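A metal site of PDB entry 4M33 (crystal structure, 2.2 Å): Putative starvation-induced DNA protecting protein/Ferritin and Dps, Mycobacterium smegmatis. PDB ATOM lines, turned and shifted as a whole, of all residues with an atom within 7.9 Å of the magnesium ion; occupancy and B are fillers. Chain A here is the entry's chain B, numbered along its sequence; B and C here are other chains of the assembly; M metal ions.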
ATOM      1  N   SER A  54      19.976 -10.979 -15.050  1.00  0.00           N
ATOM      2  CA  SER A  54      18.531 -11.175 -14.847  1.00  0.00           C
ATOM      3  C   SER A  54      17.685 -10.338 -15.803  1.00  0.00           C
ATOM      4  O   SER A  54      17.797  -9.106 -15.819  1.00  0.00           O
ATOM      5  CB  SER A  54      18.125 -10.863 -13.412  1.00  0.00           C
ATOM      6  OG  SER A  54      18.998 -11.513 -12.494  1.00  0.00           O
ATOM      7  N   ASN A  55      16.844 -11.019 -16.569  1.00  0.00           N
ATOM      8  CA  ASN A  55      16.010 -10.394 -17.586  1.00  0.00           C
ATOM      9  C   ASN A  55      16.795  -9.800 -18.746  1.00  0.00           C
ATOM     10  O   ASN A  55      16.444  -8.734 -19.272  1.00  0.00           O
ATOM     11  CB  ASN A  55      15.037  -9.370 -16.982  1.00  0.00           C
ATOM     12  CG  ASN A  55      13.783  -9.214 -17.799  1.00  0.00           C
ATOM     13  OD1 ASN A  55      13.441 -10.104 -18.578  1.00  0.00           O
ATOM     14  ND2 ASN A  55      13.102  -8.087 -17.659  1.00  0.00           N
ATOM     15  N   PHE A  56      17.851 -10.506 -19.136  1.00  0.00           N
ATOM     16  CA  PHE A  56      18.628 -10.147 -20.312  1.00  0.00           C
ATOM     17  C   PHE A  56      17.738  -9.894 -21.538  1.00  0.00           C
ATOM     18  O   PHE A  56      17.779  -8.812 -22.124  1.00  0.00           O
ATOM     19  CB  PHE A  56      19.660 -11.223 -20.630  1.00  0.00           C
ATOM     20  CG  PHE A  56      20.172 -11.191 -22.041  1.00  0.00           C
ATOM     21  CD1 PHE A  56      21.116 -10.251 -22.421  1.00  0.00           C
ATOM     22  CD2 PHE A  56      19.702 -12.098 -22.979  1.00  0.00           C
ATOM     23  CE1 PHE A  56      21.591 -10.211 -23.733  1.00  0.00           C
ATOM     24  CE2 PHE A  56      20.171 -12.071 -24.293  1.00  0.00           C
ATOM     25  CZ  PHE A  56      21.115 -11.124 -24.666  1.00  0.00           C
ATOM     26  N   ARG A  57      16.921 -10.886 -21.884  1.00  0.00           N
ATOM     27  CA  ARG A  57      16.242 -10.911 -23.180  1.00  0.00           C
ATOM     28  C   ARG A  57      15.345  -9.694 -23.398  1.00  0.00           C
ATOM     29  O   ARG A  57      15.438  -9.034 -24.431  1.00  0.00           O
ATOM     30  CB  ARG A  57      15.463 -12.216 -23.377  1.00  0.00           C
ATOM     31  CG  ARG A  57      14.915 -12.414 -24.785  1.00  0.00           C
ATOM     32  CD  ARG A  57      14.137 -13.709 -24.913  1.00  0.00           C
ATOM     33  NE  ARG A  57      13.528 -13.885 -26.232  1.00  0.00           N
ATOM     34  CZ  ARG A  57      12.305 -13.454 -26.565  1.00  0.00           C
ATOM     35  NH1 ARG A  57      11.555 -12.808 -25.667  1.00  0.00           N
ATOM     36  NH2 ARG A  57      11.848 -13.660 -27.791  1.00  0.00           N
ATOM     37  N   ASP A  58      14.485  -9.404 -22.410  1.00  0.00           N
ATOM     38  CA  ASP A  58      13.630  -8.212 -22.441  1.00  0.00           C
ATOM     39  C   ASP A  58      14.408  -6.930 -22.742  1.00  0.00           C
ATOM     40  O   ASP A  58      13.990  -6.145 -23.590  1.00  0.00           O
ATOM     41  CB  ASP A  58      12.871  -8.061 -21.126  1.00  0.00           C
ATOM     42  CG  ASP A  58      11.494  -8.694 -21.165  1.00  0.00           C
ATOM     43  OD1 ASP A  58      10.904  -8.826 -22.263  1.00  0.00           O
ATOM     44  OD2 ASP A  58      11.007  -9.062 -20.076  1.00  0.00           O
ATOM     45  N   LEU A  59      15.517  -6.724 -22.043  1.00  0.00           N
ATOM     46  CA  LEU A  59      16.325  -5.520 -22.231  1.00  0.00           C
ATOM     47  C   LEU A  59      17.012  -5.507 -23.585  1.00  0.00           C
ATOM     48  O   LEU A  59      16.964  -4.500 -24.299  1.00  0.00           O
ATOM     49  CB  LEU A  59      17.337  -5.311 -21.091  1.00  0.00           C
ATOM     50  CG  LEU A  59      16.907  -4.384 -19.949  1.00  0.00           C
ATOM     51  CD1 LEU A  59      16.717  -2.932 -20.437  1.00  0.00           C
ATOM     52  CD2 LEU A  59      15.624  -4.884 -19.263  1.00  0.00           C
ATOM     53  N   GLU A 164      11.738  -1.684 -15.024  1.00  0.00           N
ATOM     54  CA  GLU A 164      12.445  -2.879 -14.556  1.00  0.00           C
ATOM     55  C   GLU A 164      13.120  -2.698 -13.180  1.00  0.00           C
ATOM     56  O   GLU A 164      13.262  -3.663 -12.428  1.00  0.00           O
ATOM     57  CB  GLU A 164      13.473  -3.294 -15.619  1.00  0.00           C
ATOM     58  CG  GLU A 164      14.469  -4.380 -15.218  1.00  0.00           C
ATOM     59  CD  GLU A 164      13.864  -5.764 -15.089  1.00  0.00           C
ATOM     60  OE1 GLU A 164      14.397  -6.563 -14.301  1.00  0.00           O
ATOM     61  OE2 GLU A 164      12.853  -6.056 -15.761  1.00  0.00           O
ATOM     62  N   SER B  54      10.855  -6.054 -11.376  1.00  0.00           N
ATOM     63  CA  SER B  54      11.595  -7.081 -12.105  1.00  0.00           C
ATOM     64  C   SER B  54      10.730  -7.842 -13.102  1.00  0.00           C
ATOM     65  O   SER B  54       9.641  -8.323 -12.764  1.00  0.00           O
ATOM     66  CB  SER B  54      12.316  -8.037 -11.161  1.00  0.00           C
ATOM     67  OG  SER B  54      11.446  -8.473 -10.137  1.00  0.00           O
ATOM     68  N   ASN B  55      11.229  -7.934 -14.333  1.00  0.00           N
ATOM     69  CA  ASN B  55      10.521  -8.529 -15.473  1.00  0.00           C
ATOM     70  C   ASN B  55       9.237  -7.789 -15.874  1.00  0.00           C
ATOM     71  O   ASN B  55       8.276  -8.407 -16.323  1.00  0.00           O
ATOM     72  CB  ASN B  55      10.269 -10.034 -15.266  1.00  0.00           C
ATOM     73  CG  ASN B  55      10.148 -10.785 -16.583  1.00  0.00           C
ATOM     74  OD1 ASN B  55      10.784 -10.408 -17.573  1.00  0.00           O
ATOM     75  ND2 ASN B  55       9.329 -11.823 -16.608  1.00  0.00           N
ATOM     76  N   PHE B  56       9.264  -6.474 -15.719  1.00  0.00           N
ATOM     77  CA  PHE B  56       8.172  -5.580 -16.127  1.00  0.00           C
ATOM     78  C   PHE B  56       7.702  -5.818 -17.572  1.00  0.00           C
ATOM     79  O   PHE B  56       6.497  -5.950 -17.821  1.00  0.00           O
ATOM     80  CB  PHE B  56       8.589  -4.105 -15.945  1.00  0.00           C
ATOM     81  CG  PHE B  56       7.852  -3.143 -16.842  1.00  0.00           C
ATOM     82  CD1 PHE B  56       8.427  -2.689 -18.018  1.00  0.00           C
ATOM     83  CD2 PHE B  56       6.585  -2.683 -16.498  1.00  0.00           C
ATOM     84  CE1 PHE B  56       7.749  -1.792 -18.852  1.00  0.00           C
ATOM     85  CE2 PHE B  56       5.901  -1.786 -17.319  1.00  0.00           C
ATOM     86  CZ  PHE B  56       6.477  -1.350 -18.495  1.00  0.00           C
ATOM     87  N   ARG B  57       8.644  -5.852 -18.514  1.00  0.00           N
ATOM     88  CA  ARG B  57       8.314  -5.883 -19.942  1.00  0.00           C
ATOM     89  C   ARG B  57       7.505  -7.116 -20.351  1.00  0.00           C
ATOM     90  O   ARG B  57       6.476  -6.985 -21.006  1.00  0.00           O
ATOM     91  CB  ARG B  57       9.580  -5.744 -20.799  1.00  0.00           C
ATOM     92  CG  ARG B  57       9.319  -5.613 -22.285  1.00  0.00           C
ATOM     93  CD  ARG B  57      10.631  -5.422 -23.032  1.00  0.00           C
ATOM     94  NE  ARG B  57      10.431  -5.258 -24.470  1.00  0.00           N
ATOM     95  CZ  ARG B  57      10.404  -6.265 -25.340  1.00  0.00           C
ATOM     96  NH1 ARG B  57      10.548  -7.517 -24.935  1.00  0.00           N
ATOM     97  NH2 ARG B  57      10.221  -6.010 -26.635  1.00  0.00           N
ATOM     98  N   ASP B  58       7.984  -8.299 -19.970  1.00  0.00           N
ATOM     99  CA  ASP B  58       7.289  -9.552 -20.239  1.00  0.00           C
ATOM    100  C   ASP B  58       5.840  -9.483 -19.774  1.00  0.00           C
ATOM    101  O   ASP B  58       4.924  -9.868 -20.505  1.00  0.00           O
ATOM    102  CB  ASP B  58       7.974 -10.736 -19.559  1.00  0.00           C
ATOM    103  CG  ASP B  58       8.934 -11.470 -20.462  1.00  0.00           C
ATOM    104  OD1 ASP B  58       8.693 -11.544 -21.692  1.00  0.00           O
ATOM    105  OD2 ASP B  58       9.932 -11.978 -19.937  1.00  0.00           O
ATOM    106  N   LEU B  59       5.654  -9.008 -18.549  1.00  0.00           N
ATOM    107  CA  LEU B  59       4.321  -8.874 -17.975  1.00  0.00           C
ATOM    108  C   LEU B  59       3.493  -7.805 -18.682  1.00  0.00           C
ATOM    109  O   LEU B  59       2.336  -8.055 -19.033  1.00  0.00           O
ATOM    110  CB  LEU B  59       4.392  -8.640 -16.466  1.00  0.00           C
ATOM    111  CG  LEU B  59       4.183  -9.899 -15.610  1.00  0.00           C
ATOM    112  CD1 LEU B  59       2.789 -10.493 -15.847  1.00  0.00           C
ATOM    113  CD2 LEU B  59       5.270 -10.943 -15.867  1.00  0.00           C
ATOM    114  N   GLU B 164       5.548 -17.042 -13.729  1.00  0.00           N
ATOM    115  CA  GLU B 164       6.552 -16.066 -13.291  1.00  0.00           C
ATOM    116  C   GLU B 164       6.870 -16.172 -11.790  1.00  0.00           C
ATOM    117  O   GLU B 164       8.012 -15.998 -11.390  1.00  0.00           O
ATOM    118  CB  GLU B 164       6.075 -14.642 -13.636  1.00  0.00           C
ATOM    119  CG  GLU B 164       6.877 -13.501 -12.985  1.00  0.00           C
ATOM    120  CD  GLU B 164       8.334 -13.401 -13.472  1.00  0.00           C
ATOM    121  OE1 GLU B 164       8.648 -13.811 -14.614  1.00  0.00           O
ATOM    122  OE2 GLU B 164       9.159 -12.884 -12.688  1.00  0.00           O
ATOM    123  N   SER C  54      11.226 -17.121 -12.247  1.00  0.00           N
ATOM    124  CA  SER C  54      11.620 -15.774 -12.630  1.00  0.00           C
ATOM    125  C   SER C  54      12.006 -15.649 -14.110  1.00  0.00           C
ATOM    126  O   SER C  54      12.859 -16.394 -14.597  1.00  0.00           O
ATOM    127  CB  SER C  54      12.766 -15.303 -11.737  1.00  0.00           C
ATOM    128  OG  SER C  54      13.047 -13.935 -11.937  1.00  0.00           O
ATOM    129  N   ASN C  55      11.366 -14.711 -14.799  1.00  0.00           N
ATOM    130  CA  ASN C  55      11.569 -14.486 -16.232  1.00  0.00           C
ATOM    131  C   ASN C  55      11.159 -15.679 -17.096  1.00  0.00           C
ATOM    132  O   ASN C  55      11.784 -15.962 -18.128  1.00  0.00           O
ATOM    133  CB  ASN C  55      13.010 -14.059 -16.547  1.00  0.00           C
ATOM    134  CG  ASN C  55      13.105 -13.262 -17.834  1.00  0.00           C
ATOM    135  OD1 ASN C  55      12.137 -12.622 -18.248  1.00  0.00           O
ATOM    136  ND2 ASN C  55      14.274 -13.277 -18.469  1.00  0.00           N
ATOM    137  N   PHE C  56      10.104 -16.373 -16.665  1.00  0.00           N
ATOM    138  CA  PHE C  56       9.525 -17.489 -17.401  1.00  0.00           C
ATOM    139  C   PHE C  56       9.267 -17.153 -18.873  1.00  0.00           C
ATOM    140  O   PHE C  56       9.651 -17.914 -19.760  1.00  0.00           O
ATOM    141  CB  PHE C  56       8.203 -17.937 -16.754  1.00  0.00           C
ATOM    142  CG  PHE C  56       7.285 -18.666 -17.696  1.00  0.00           C
ATOM    143  CD1 PHE C  56       7.493 -20.015 -17.990  1.00  0.00           C
ATOM    144  CD2 PHE C  56       6.219 -18.012 -18.297  1.00  0.00           C
ATOM    145  CE1 PHE C  56       6.651 -20.697 -18.871  1.00  0.00           C
ATOM    146  CE2 PHE C  56       5.374 -18.683 -19.186  1.00  0.00           C
ATOM    147  CZ  PHE C  56       5.591 -20.031 -19.469  1.00  0.00           C
ATOM    148  N   ARG C  57       8.612 -16.028 -19.119  1.00  0.00           N
ATOM    149  CA  ARG C  57       8.088 -15.701 -20.441  1.00  0.00           C
ATOM    150  C   ARG C  57       9.192 -15.549 -21.479  1.00  0.00           C
ATOM    151  O   ARG C  57       9.118 -16.154 -22.557  1.00  0.00           O
ATOM    152  CB  ARG C  57       7.197 -14.450 -20.388  1.00  0.00           C
ATOM    153  CG  ARG C  57       6.437 -14.176 -21.691  1.00  0.00           C
ATOM    154  CD  ARG C  57       5.654 -12.883 -21.603  1.00  0.00           C
ATOM    155  NE  ARG C  57       4.955 -12.570 -22.850  1.00  0.00           N
ATOM    156  CZ  ARG C  57       5.418 -11.773 -23.810  1.00  0.00           C
ATOM    157  NH1 ARG C  57       6.612 -11.195 -23.678  1.00  0.00           N
ATOM    158  NH2 ARG C  57       4.694 -11.552 -24.891  1.00  0.00           N
ATOM    159  N   ASP C  58      10.222 -14.774 -21.150  1.00  0.00           N
ATOM    160  CA  ASP C  58      11.383 -14.624 -22.035  1.00  0.00           C
ATOM    161  C   ASP C  58      11.997 -15.961 -22.453  1.00  0.00           C
ATOM    162  O   ASP C  58      12.285 -16.166 -23.632  1.00  0.00           O
ATOM    163  CB  ASP C  58      12.472 -13.766 -21.376  1.00  0.00           C
ATOM    164  CG  ASP C  58      12.389 -12.308 -21.758  1.00  0.00           C
ATOM    165  OD1 ASP C  58      12.061 -11.997 -22.922  1.00  0.00           O
ATOM    166  OD2 ASP C  58      12.663 -11.460 -20.877  1.00  0.00           O
ATOM    167  N   LEU C  59      12.204 -16.855 -21.491  1.00  0.00           N
ATOM    168  CA  LEU C  59      12.827 -18.137 -21.799  1.00  0.00           C
ATOM    169  C   LEU C  59      11.895 -19.061 -22.569  1.00  0.00           C
ATOM    170  O   LEU C  59      12.317 -19.755 -23.487  1.00  0.00           O
ATOM    171  CB  LEU C  59      13.350 -18.816 -20.527  1.00  0.00           C
ATOM    172  CG  LEU C  59      14.830 -18.562 -20.174  1.00  0.00           C
ATOM    173  CD1 LEU C  59      15.761 -19.066 -21.275  1.00  0.00           C
ATOM    174  CD2 LEU C  59      15.109 -17.088 -19.841  1.00  0.00           C
ATOM    175  N   GLU C 164      21.061 -14.776 -19.379  1.00  0.00           N
ATOM    176  CA  GLU C 164      20.170 -14.671 -18.225  1.00  0.00           C
ATOM    177  C   GLU C 164      20.871 -14.955 -16.885  1.00  0.00           C
ATOM    178  O   GLU C 164      20.598 -14.287 -15.890  1.00  0.00           O
ATOM    179  CB  GLU C 164      18.961 -15.609 -18.412  1.00  0.00           C
ATOM    180  CG  GLU C 164      18.076 -15.813 -17.176  1.00  0.00           C
ATOM    181  CD  GLU C 164      17.276 -14.579 -16.779  1.00  0.00           C
ATOM    182  OE1 GLU C 164      16.948 -14.446 -15.578  1.00  0.00           O
ATOM    183  OE2 GLU C 164      16.978 -13.737 -17.655  1.00  0.00           O
HETATM  184 MG    MG M   1      11.594 -10.962 -19.220  1.00  0.00          MG
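OE1 of Glu 164 of chain B lies within hydrogen-bond range of ND2 of Asn 55 of chain B (2.9 Å).
N of Asn 55 of chain C is in hydrogen-bond range of OE1 of Glu 164 of chain B, at 2.9 Å.
The side-chain carboxylate (OE2) of Glu 164 of chain C sits at hydrogen-bond distance from the side-chain amide nitrogen (ND2) of Asn 55 of chain C, 2.9 Å away.
NH1 of Arg 57 of chain A is in salt-bridge range of OD1 of Asp 58 of chain C (2.9 Å).
OD1 of Asp 58 of chain B lies within salt-bridge range of NH1 of Arg 57 of chain C, 2.9 Å away.
OE2 of Glu 164 of chain A is in hydrogen-bond range of ND2 of Asn 55 of chain A, 2.8 Å away.
N of Asn 55 of chain A is in hydrogen-bond range of OE2 of Glu 164 of chain C (2.9 Å).
NH1 of Arg 57 of chain B is in salt-bridge range of OD1 of Asp 58 of chain A, at 3.0 Å.
Six residues have an atom within 4 Å of the magnesium ion: Asn 55 of chain A, Asp 58 of chain A, Asn 55 of chain B, Asp 58 of chain B, Asn 55 of chain C and Asp 58 of chain C.
Along chain A the residues within 4 Å of the magnesium ion span positions 55 to 58.
The nearest printed residue that does not touch the magnesium ion is Arg 57 of chain C (5.6 Å).
The magnesium ion is bound by the side-chain amide oxygen (OD1) of Asn 55 of chain B (1.9 Å), the side-chain amide oxygen (OD1) of Asn 55 of chain C (2.0 Å), the side-chain carboxylate (OD2) of Asp 58 of chain C (2.0 Å), the side-chain carboxylate (OD2) of Asp 58 of chain B (2.1 Å), the side-chain amide oxygen (OD1) of Asn 55 of chain A (2.1 Å) and the side-chain carboxylate (OD2) of Asp 58 of chain A (2.2 Å).
The magnesium ion has six donor atoms within binding distance.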
